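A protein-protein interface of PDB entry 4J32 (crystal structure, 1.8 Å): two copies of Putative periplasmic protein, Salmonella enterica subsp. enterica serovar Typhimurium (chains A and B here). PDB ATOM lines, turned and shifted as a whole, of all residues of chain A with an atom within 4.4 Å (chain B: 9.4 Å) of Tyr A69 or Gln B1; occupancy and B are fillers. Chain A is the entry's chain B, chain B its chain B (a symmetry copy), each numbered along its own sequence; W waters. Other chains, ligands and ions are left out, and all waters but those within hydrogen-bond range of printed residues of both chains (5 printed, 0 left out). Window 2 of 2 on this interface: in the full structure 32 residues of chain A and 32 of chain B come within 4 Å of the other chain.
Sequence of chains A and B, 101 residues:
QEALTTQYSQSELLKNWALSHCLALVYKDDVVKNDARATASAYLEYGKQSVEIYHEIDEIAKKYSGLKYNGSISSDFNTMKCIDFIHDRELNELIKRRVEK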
ATOM      1  N   LEU A  67     -17.712 -11.829  -5.352  1.00  0.00           N
ATOM      2  CA  LEU A  67     -18.681 -11.319  -4.365  1.00  0.00           C
ATOM      3  C   LEU A  67     -19.618 -10.294  -4.996  1.00  0.00           C
ATOM      4  O   LEU A  67     -19.260  -9.609  -5.970  1.00  0.00           O
ATOM      5  CB  LEU A  67     -17.960 -10.697  -3.157  1.00  0.00           C
ATOM      6  CG  LEU A  67     -17.097 -11.614  -2.258  1.00  0.00           C
ATOM      7  CD1 LEU A  67     -16.357 -10.811  -1.192  1.00  0.00           C
ATOM      8  CD2 LEU A  67     -17.926 -12.702  -1.621  1.00  0.00           C
ATOM      9  N   LYS A  68     -20.822 -10.184  -4.443  1.00  0.00           N
ATOM     10  CA  LYS A  68     -21.712  -9.082  -4.817  1.00  0.00           C
ATOM     11  C   LYS A  68     -21.803  -8.140  -3.638  1.00  0.00           C
ATOM     12  O   LYS A  68     -22.285  -8.531  -2.572  1.00  0.00           O
ATOM     13  CB  LYS A  68     -23.110  -9.588  -5.202  1.00  0.00           C
ATOM     14  CG  LYS A  68     -23.102 -10.656  -6.310  1.00  0.00           C
ATOM     15  CD  LYS A  68     -22.494 -10.148  -7.624  1.00  0.00           C
ATOM     16  CE  LYS A  68     -22.003 -11.323  -8.464  1.00  0.00           C
ATOM     17  NZ  LYS A  68     -22.198 -11.099  -9.932  1.00  0.00           N
ATOM     18  N   TYR A  69     -21.337  -6.906  -3.837  1.00  0.00           N
ATOM     19  CA  TYR A  69     -21.400  -5.873  -2.811  1.00  0.00           C
ATOM     20  C   TYR A  69     -22.474  -4.834  -3.161  1.00  0.00           C
ATOM     21  O   TYR A  69     -22.596  -4.425  -4.315  1.00  0.00           O
ATOM     22  CB  TYR A  69     -20.046  -5.158  -2.687  1.00  0.00           C
ATOM     23  CG  TYR A  69     -18.966  -5.885  -1.912  1.00  0.00           C
ATOM     24  CD1 TYR A  69     -17.648  -5.373  -1.879  1.00  0.00           C
ATOM     25  CD2 TYR A  69     -19.249  -7.043  -1.162  1.00  0.00           C
ATOM     26  CE1 TYR A  69     -16.638  -6.009  -1.142  1.00  0.00           C
ATOM     27  CE2 TYR A  69     -18.232  -7.692  -0.428  1.00  0.00           C
ATOM     28  CZ  TYR A  69     -16.941  -7.158  -0.415  1.00  0.00           C
ATOM     29  OH  TYR A  69     -15.949  -7.783   0.330  1.00  0.00           O
ATOM     30  N   ASN A  70     -23.212  -4.404  -2.149  1.00  0.00           N
ATOM     31  CA  ASN A  70     -24.328  -3.468  -2.322  1.00  0.00           C
ATOM     32  C   ASN A  70     -24.193  -2.288  -1.355  1.00  0.00           C
ATOM     33  O   ASN A  70     -23.491  -2.380  -0.349  1.00  0.00           O
ATOM     34  CB  ASN A  70     -25.646  -4.210  -2.087  1.00  0.00           C
ATOM     35  CG  ASN A  70     -25.826  -5.389  -3.037  1.00  0.00           C
ATOM     36  OD1 ASN A  70     -26.093  -5.190  -4.230  1.00  0.00           O
ATOM     37  ND2 ASN A  70     -25.677  -6.626  -2.517  1.00  0.00           N
ATOM     38  N   SER A  75     -23.510   1.474  -7.181  1.00  0.00           N
ATOM     39  CA  SER A  75     -22.161   0.985  -7.469  1.00  0.00           C
ATOM     40  C   SER A  75     -22.135  -0.518  -7.259  1.00  0.00           C
ATOM     41  O   SER A  75     -22.913  -1.061  -6.467  1.00  0.00           O
ATOM     42  CB  SER A  75     -21.136   1.637  -6.527  1.00  0.00           C
ATOM     43  OG  SER A  75     -19.809   1.280  -6.892  1.00  0.00           O
ATOM     44  N   ASP A  76     -21.245  -1.176  -7.986  1.00  0.00           N
ATOM     45  CA  ASP A  76     -20.940  -2.570  -7.718  1.00  0.00           C
ATOM     46  C   ASP A  76     -19.844  -2.715  -6.668  1.00  0.00           C
ATOM     47  O   ASP A  76     -19.546  -3.835  -6.227  1.00  0.00           O
ATOM     48  CB  ASP A  76     -20.531  -3.256  -9.018  1.00  0.00           C
ATOM     49  CG  ASP A  76     -21.701  -3.447  -9.957  1.00  0.00           C
ATOM     50  OD1 ASP A  76     -22.841  -3.549  -9.480  1.00  0.00           O
ATOM     51  OD2 ASP A  76     -21.477  -3.525 -11.178  1.00  0.00           O
ATOM     52  N   PHE A  77     -19.224  -1.601  -6.291  1.00  0.00           N
ATOM     53  CA  PHE A  77     -18.086  -1.625  -5.336  1.00  0.00           C
ATOM     54  C   PHE A  77     -16.966  -2.643  -5.698  1.00  0.00           C
ATOM     55  O   PHE A  77     -16.424  -3.330  -4.820  1.00  0.00           O
ATOM     56  CB  PHE A  77     -18.617  -1.848  -3.906  1.00  0.00           C
ATOM     57  CG  PHE A  77     -19.504  -0.724  -3.417  1.00  0.00           C
ATOM     58  CD1 PHE A  77     -18.941   0.472  -2.960  1.00  0.00           C
ATOM     59  CD2 PHE A  77     -20.893  -0.865  -3.406  1.00  0.00           C
ATOM     60  CE1 PHE A  77     -19.767   1.515  -2.495  1.00  0.00           C
ATOM     61  CE2 PHE A  77     -21.722   0.183  -2.941  1.00  0.00           C
ATOM     62  CZ  PHE A  77     -21.145   1.369  -2.493  1.00  0.00           C
ATOM     63  N   MET A  80     -13.695  -2.085  -3.961  1.00  0.00           N
ATOM     64  CA  MET A  80     -13.782  -2.536  -2.568  1.00  0.00           C
ATOM     65  C   MET A  80     -13.489  -4.026  -2.381  1.00  0.00           C
ATOM     66  O   MET A  80     -12.950  -4.452  -1.328  1.00  0.00           O
ATOM     67  CB  MET A  80     -15.177  -2.231  -2.022  1.00  0.00           C
ATOM     68  CG  MET A  80     -15.269  -2.417  -0.540  1.00  0.00           C
ATOM     69  SD  MET A  80     -16.896  -1.935   0.105  1.00  0.00           S
ATOM     70  CE  MET A  80     -16.689  -0.149   0.177  1.00  0.00           C
ATOM     71  N   LYS A  81     -13.898  -4.839  -3.355  1.00  0.00           N
ATOM     72  CA  LYS A  81     -13.630  -6.285  -3.294  1.00  0.00           C
ATOM     73  C   LYS A  81     -12.109  -6.513  -3.180  1.00  0.00           C
ATOM     74  O   LYS A  81     -11.654  -7.352  -2.383  1.00  0.00           O
ATOM     75  CB  LYS A  81     -14.217  -6.996  -4.527  1.00  0.00           C
ATOM     76  CG  LYS A  81     -15.735  -6.826  -4.634  1.00  0.00           C
ATOM     77  CD  LYS A  81     -16.287  -7.280  -5.976  1.00  0.00           C
ATOM     78  CE  LYS A  81     -17.731  -6.777  -6.114  1.00  0.00           C
ATOM     79  NZ  LYS A  81     -18.310  -7.222  -7.439  1.00  0.00           N
ATOM     80  N   ASP A  84     -10.704  -5.295   0.256  1.00  0.00           N
ATOM     81  CA  ASP A  84     -10.973  -6.320   1.269  1.00  0.00           C
ATOM     82  C   ASP A  84     -10.020  -7.508   1.052  1.00  0.00           C
ATOM     83  O   ASP A  84      -9.496  -8.099   2.018  1.00  0.00           O
ATOM     84  CB  ASP A  84     -12.437  -6.782   1.204  1.00  0.00           C
ATOM     85  CG  ASP A  84     -13.414  -5.753   1.795  1.00  0.00           C
ATOM     86  OD1 ASP A  84     -12.962  -4.762   2.440  1.00  0.00           O
ATOM     87  OD2 ASP A  84     -14.644  -5.978   1.664  1.00  0.00           O
ATOM     88  N   GLN B   1     -23.806  -9.711   0.012  1.00  0.00           N
ATOM     89  CA  GLN B   1     -22.716  -9.835   0.999  1.00  0.00           C
ATOM     90  C   GLN B   1     -22.343  -8.430   1.472  1.00  0.00           C
ATOM     91  O   GLN B   1     -22.151  -7.509   0.667  1.00  0.00           O
ATOM     92  CB  GLN B   1     -21.532 -10.589   0.369  1.00  0.00           C
ATOM     93  CG  GLN B   1     -21.788 -12.117   0.212  1.00  0.00           C
ATOM     94  CD  GLN B   1     -21.417 -12.714  -1.160  1.00  0.00           C
ATOM     95  OE1 GLN B   1     -21.496 -12.054  -2.202  1.00  0.00           O
ATOM     96  NE2 GLN B   1     -21.052 -14.000  -1.154  1.00  0.00           N
ATOM     97  N   GLU B   2     -22.281  -8.239   2.792  1.00  0.00           N
ATOM     98  CA  GLU B   2     -21.781  -6.941   3.288  1.00  0.00           C
ATOM     99  C   GLU B   2     -20.255  -6.967   3.223  1.00  0.00           C
ATOM    100  O   GLU B   2     -19.648  -7.973   3.602  1.00  0.00           O
ATOM    101  CB  GLU B   2     -22.244  -6.637   4.717  1.00  0.00           C
ATOM    102  CG  GLU B   2     -21.877  -5.219   5.156  1.00  0.00           C
ATOM    103  CD  GLU B   2     -22.401  -4.837   6.529  1.00  0.00           C
ATOM    104  OE1 GLU B   2     -21.667  -4.125   7.245  1.00  0.00           O
ATOM    105  OE2 GLU B   2     -23.534  -5.224   6.888  1.00  0.00           O
ATOM    106  N   ALA B   3     -19.635  -5.883   2.744  1.00  0.00           N
ATOM    107  CA  ALA B   3     -18.174  -5.776   2.698  1.00  0.00           C
ATOM    108  C   ALA B   3     -17.592  -5.657   4.098  1.00  0.00           C
ATOM    109  O   ALA B   3     -18.332  -5.572   5.092  1.00  0.00           O
ATOM    110  CB  ALA B   3     -17.746  -4.583   1.850  1.00  0.00           C
ATOM    111  N   LEU B   4     -16.265  -5.649   4.183  1.00  0.00           N
ATOM    112  CA  LEU B   4     -15.576  -5.597   5.473  1.00  0.00           C
ATOM    113  C   LEU B   4     -15.432  -4.200   6.054  1.00  0.00           C
ATOM    114  O   LEU B   4     -14.713  -4.016   7.043  1.00  0.00           O
ATOM    115  CB  LEU B   4     -14.196  -6.244   5.364  1.00  0.00           C
ATOM    116  CG  LEU B   4     -14.217  -7.694   4.885  1.00  0.00           C
ATOM    117  CD1 LEU B   4     -12.765  -8.219   4.742  1.00  0.00           C
ATOM    118  CD2 LEU B   4     -15.081  -8.615   5.754  1.00  0.00           C
ATOM    119  N   THR B   5     -16.111  -3.220   5.447  1.00  0.00           N
ATOM    120  CA  THR B   5     -15.875  -1.805   5.738  1.00  0.00           C
ATOM    121  C   THR B   5     -15.869  -1.459   7.239  1.00  0.00           C
ATOM    122  O   THR B   5     -15.028  -0.686   7.681  1.00  0.00           O
ATOM    123  CB  THR B   5     -16.899  -0.932   4.973  1.00  0.00           C
ATOM    124  OG1 THR B   5     -17.079  -1.494   3.654  1.00  0.00           O
ATOM    125  CG2 THR B   5     -16.404   0.527   4.834  1.00  0.00           C
ATOM    126  N   GLN B   7     -14.997  -3.179   9.740  1.00  0.00           N
ATOM    127  CA  GLN B   7     -13.980  -3.879  10.516  1.00  0.00           C
ATOM    128  C   GLN B   7     -12.643  -3.132  10.572  1.00  0.00           C
ATOM    129  O   GLN B   7     -11.782  -3.452  11.414  1.00  0.00           O
ATOM    130  CB  GLN B   7     -13.812  -5.315  10.001  1.00  0.00           C
ATOM    131  CG  GLN B   7     -15.021  -6.206  10.315  1.00  0.00           C
ATOM    132  CD  GLN B   7     -14.963  -7.573   9.646  1.00  0.00           C
ATOM    133  OE1 GLN B   7     -13.909  -8.212   9.576  1.00  0.00           O
ATOM    134  NE2 GLN B   7     -16.106  -8.031   9.153  1.00  0.00           N
ATOM    135  N   TYR B   8     -12.485  -2.141   9.703  1.00  0.00           N
ATOM    136  CA  TYR B   8     -11.231  -1.391   9.602  1.00  0.00           C
ATOM    137  C   TYR B   8     -11.055  -0.386  10.743  1.00  0.00           C
ATOM    138  O   TYR B   8     -12.015   0.270  11.170  1.00  0.00           O
ATOM    139  CB  TYR B   8     -11.139  -0.674   8.245  1.00  0.00           C
ATOM    140  CG  TYR B   8     -11.046  -1.656   7.089  1.00  0.00           C
ATOM    141  CD1 TYR B   8      -9.912  -2.455   6.923  1.00  0.00           C
ATOM    142  CD2 TYR B   8     -12.086  -1.755   6.152  1.00  0.00           C
ATOM    143  CE1 TYR B   8      -9.817  -3.382   5.864  1.00  0.00           C
ATOM    144  CE2 TYR B   8     -12.008  -2.681   5.080  1.00  0.00           C
ATOM    145  CZ  TYR B   8     -10.870  -3.473   4.951  1.00  0.00           C
ATOM    146  OH  TYR B   8     -10.788  -4.375   3.910  1.00  0.00           O
ATOM    147  N   ASP B  35     -16.769   3.845  -9.671  1.00  0.00           N
ATOM    148  CA  ASP B  35     -16.680   2.727  -8.737  1.00  0.00           C
ATOM    149  C   ASP B  35     -15.641   3.004  -7.642  1.00  0.00           C
ATOM    150  O   ASP B  35     -15.906   2.810  -6.443  1.00  0.00           O
ATOM    151  CB  ASP B  35     -16.296   1.456  -9.509  1.00  0.00           C
ATOM    152  CG  ASP B  35     -16.289   0.220  -8.616  1.00  0.00           C
ATOM    153  OD1 ASP B  35     -17.266  -0.562  -8.695  1.00  0.00           O
ATOM    154  OD2 ASP B  35     -15.317   0.070  -7.838  1.00  0.00           O
ATOM    155  N   THR B  39     -16.410   3.621  -3.696  1.00  0.00           N
ATOM    156  CA  THR B  39     -15.645   2.845  -2.731  1.00  0.00           C
ATOM    157  C   THR B  39     -14.941   3.783  -1.736  1.00  0.00           C
ATOM    158  O   THR B  39     -15.023   3.587  -0.515  1.00  0.00           O
ATOM    159  CB  THR B  39     -14.633   1.914  -3.468  1.00  0.00           C
ATOM    160  OG1 THR B  39     -15.362   0.940  -4.230  1.00  0.00           O
ATOM    161  CG2 THR B  39     -13.696   1.194  -2.473  1.00  0.00           C
ATOM    162  N   ALA B  42     -17.239   5.163   0.943  1.00  0.00           N
ATOM    163  CA  ALA B  42     -17.568   4.211   2.014  1.00  0.00           C
ATOM    164  C   ALA B  42     -16.561   4.349   3.162  1.00  0.00           C
ATOM    165  O   ALA B  42     -16.935   4.352   4.349  1.00  0.00           O
ATOM    166  CB  ALA B  42     -17.584   2.776   1.476  1.00  0.00           C
ATOM    167  N   TYR B  43     -15.275   4.472   2.823  1.00  0.00           N
ATOM    168  CA  TYR B  43     -14.255   4.640   3.883  1.00  0.00           C
ATOM    169  C   TYR B  43     -14.363   6.001   4.578  1.00  0.00           C
ATOM    170  O   TYR B  43     -14.120   6.093   5.791  1.00  0.00           O
ATOM    171  CB  TYR B  43     -12.843   4.402   3.337  1.00  0.00           C
ATOM    172  CG  TYR B  43     -12.744   3.022   2.740  1.00  0.00           C
ATOM    173  CD1 TYR B  43     -13.095   1.899   3.501  1.00  0.00           C
ATOM    174  CD2 TYR B  43     -12.358   2.842   1.403  1.00  0.00           C
ATOM    175  CE1 TYR B  43     -13.055   0.600   2.967  1.00  0.00           C
ATOM    176  CE2 TYR B  43     -12.298   1.542   0.849  1.00  0.00           C
ATOM    177  CZ  TYR B  43     -12.641   0.441   1.639  1.00  0.00           C
ATOM    178  OH  TYR B  43     -12.624  -0.821   1.126  1.00  0.00           O
HETATM  179  O   HOH W   1     -14.328  -2.411   2.612  1.00  0.00           O
HETATM  180  O   HOH W   2     -25.717  -7.275   0.775  1.00  0.00           O
HETATM  181  O   HOH W   3     -19.978   3.172  -8.865  1.00  0.00           O
HETATM  182  O   HOH W   4     -22.929  -5.182   0.383  1.00  0.00           O
HETATM  183  O   HOH W   5     -19.476  -0.154 -10.121  1.00  0.00           O
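Gln B1 touches Leu A67 (NE2 to CD2, 3.4 Å).
CD2 of Tyr A69 touches O of Gln B1 (3.5 Å).
CE1 of Tyr A69 touches CB of Ala B3 (3.5 Å).
OG of Ser A75 touches OD1 of Asp B35, 3.6 Å away.
OD1 of Asp B35 touches C of Asp A76 (3.9 Å).
Phe A77 touches Thr B39.
Met A80 touches Ala B3.
Ala B42 touches Met A80.
Tyr B43 touches Met A80 (OH to CG, 3.5 Å).
Asp A84 touches Ala B3 (OD2 to CB, 3.4 Å).
Hydrophobic or aromatic side chains of chain B that line the printed part of chain A: Ala B3, Leu B4, Tyr B8, Ala B42 and Tyr B43.
Among the printed residues, no Asp or Glu carboxylate lies within 4 Å of a Lys or Arg side-chain nitrogen of the other chain.
Water W4 lies within hydrogen-bond range of the backbone carbonyl oxygen of Gln B1 and the backbone NH of Asn A70.
Water W5 lies within hydrogen-bond range of OD1 of Asp B35 (2.7 Å) and N of Asp A76 (3.0 Å).
Water W1 lies within hydrogen-bond range of OD1 of Asp A84 (2.7 Å), OH of Tyr B43 (2.8 Å), OG1 of Thr B5 (3.1 Å) and SD of Met A80 (3.6 Å).
Water W3 lies within hydrogen-bond range of the side-chain hydroxyl of Ser A75 (2.7 Å) and the backbone NH of Asp B35 (3.4 Å).
Water W2 bridges the backbone NH of Gln B1 and the side-chain amide nitrogen of Asn A70.
No residue of chain B comes within 4 Å of Asn A70.
Printed residues of chain B within 4 Å of Met A80: Ala B3 (3.3 Å), Thr B5 (3.6 Å), Thr B39 (3.5 Å), Ala B42 (3.3 Å) and Tyr B43 (3.5 Å).
No residue of chain B comes within 4 Å of Lys A81.
Of the printed residues of chain A, Gln B1 touches Leu A67 (3.4 Å), Lys A68 (3.0 Å) and Tyr A69 (3.5 Å).
Glu B2 touches none of the printed residues of chain A.
Of the printed residues of chain A, Thr B39 touches Phe A77 and Met A80.
Printed residues of chain A within 4 Å of Tyr B43: Met A80.
The side-chain hydroxyl (OH) of Tyr A69 lies within hydrogen-bond range of the side-chain carboxylate (OD2) of Asp A84, at 2.6 Å.
OG1 of Thr B39 sits at hydrogen-bond distance from O of Asp B35 (2.9 Å).
The backbone carbonyl oxygen (O) of Leu A67 lies within hydrogen-bond range of the side-chain amino group (NZ) of Lys A81, at 3.0 Å.
The side-chain hydroxyl (OG) of Ser A75 is in hydrogen-bond range of the backbone NH (N) of Phe A77 (3.0 Å).
No position is printed for both chains.
N of Lys A68 is in hydrogen-bond range of OE1 of Gln B1 (3.0 Å).
The backbone NH of Phe A77 sits at hydrogen-bond distance from the side-chain carboxylate of Asp B35 (3.3 Å).
OG1 of Thr B39 is in hydrogen-bond range of N of Met A80.
The side-chain hydroxyl (OH) of Tyr B8 is in hydrogen-bond range of the side-chain carboxylate (OD1) of Asp A84, 2.7 Å away.
OD2 of Asp A84 sits at hydrogen-bond distance from N of Leu B4 (3.0 Å).
The side-chain sulfur of Met A80 lies within hydrogen-bond range of the side-chain hydroxyl of Thr B5 (3.6 Å).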
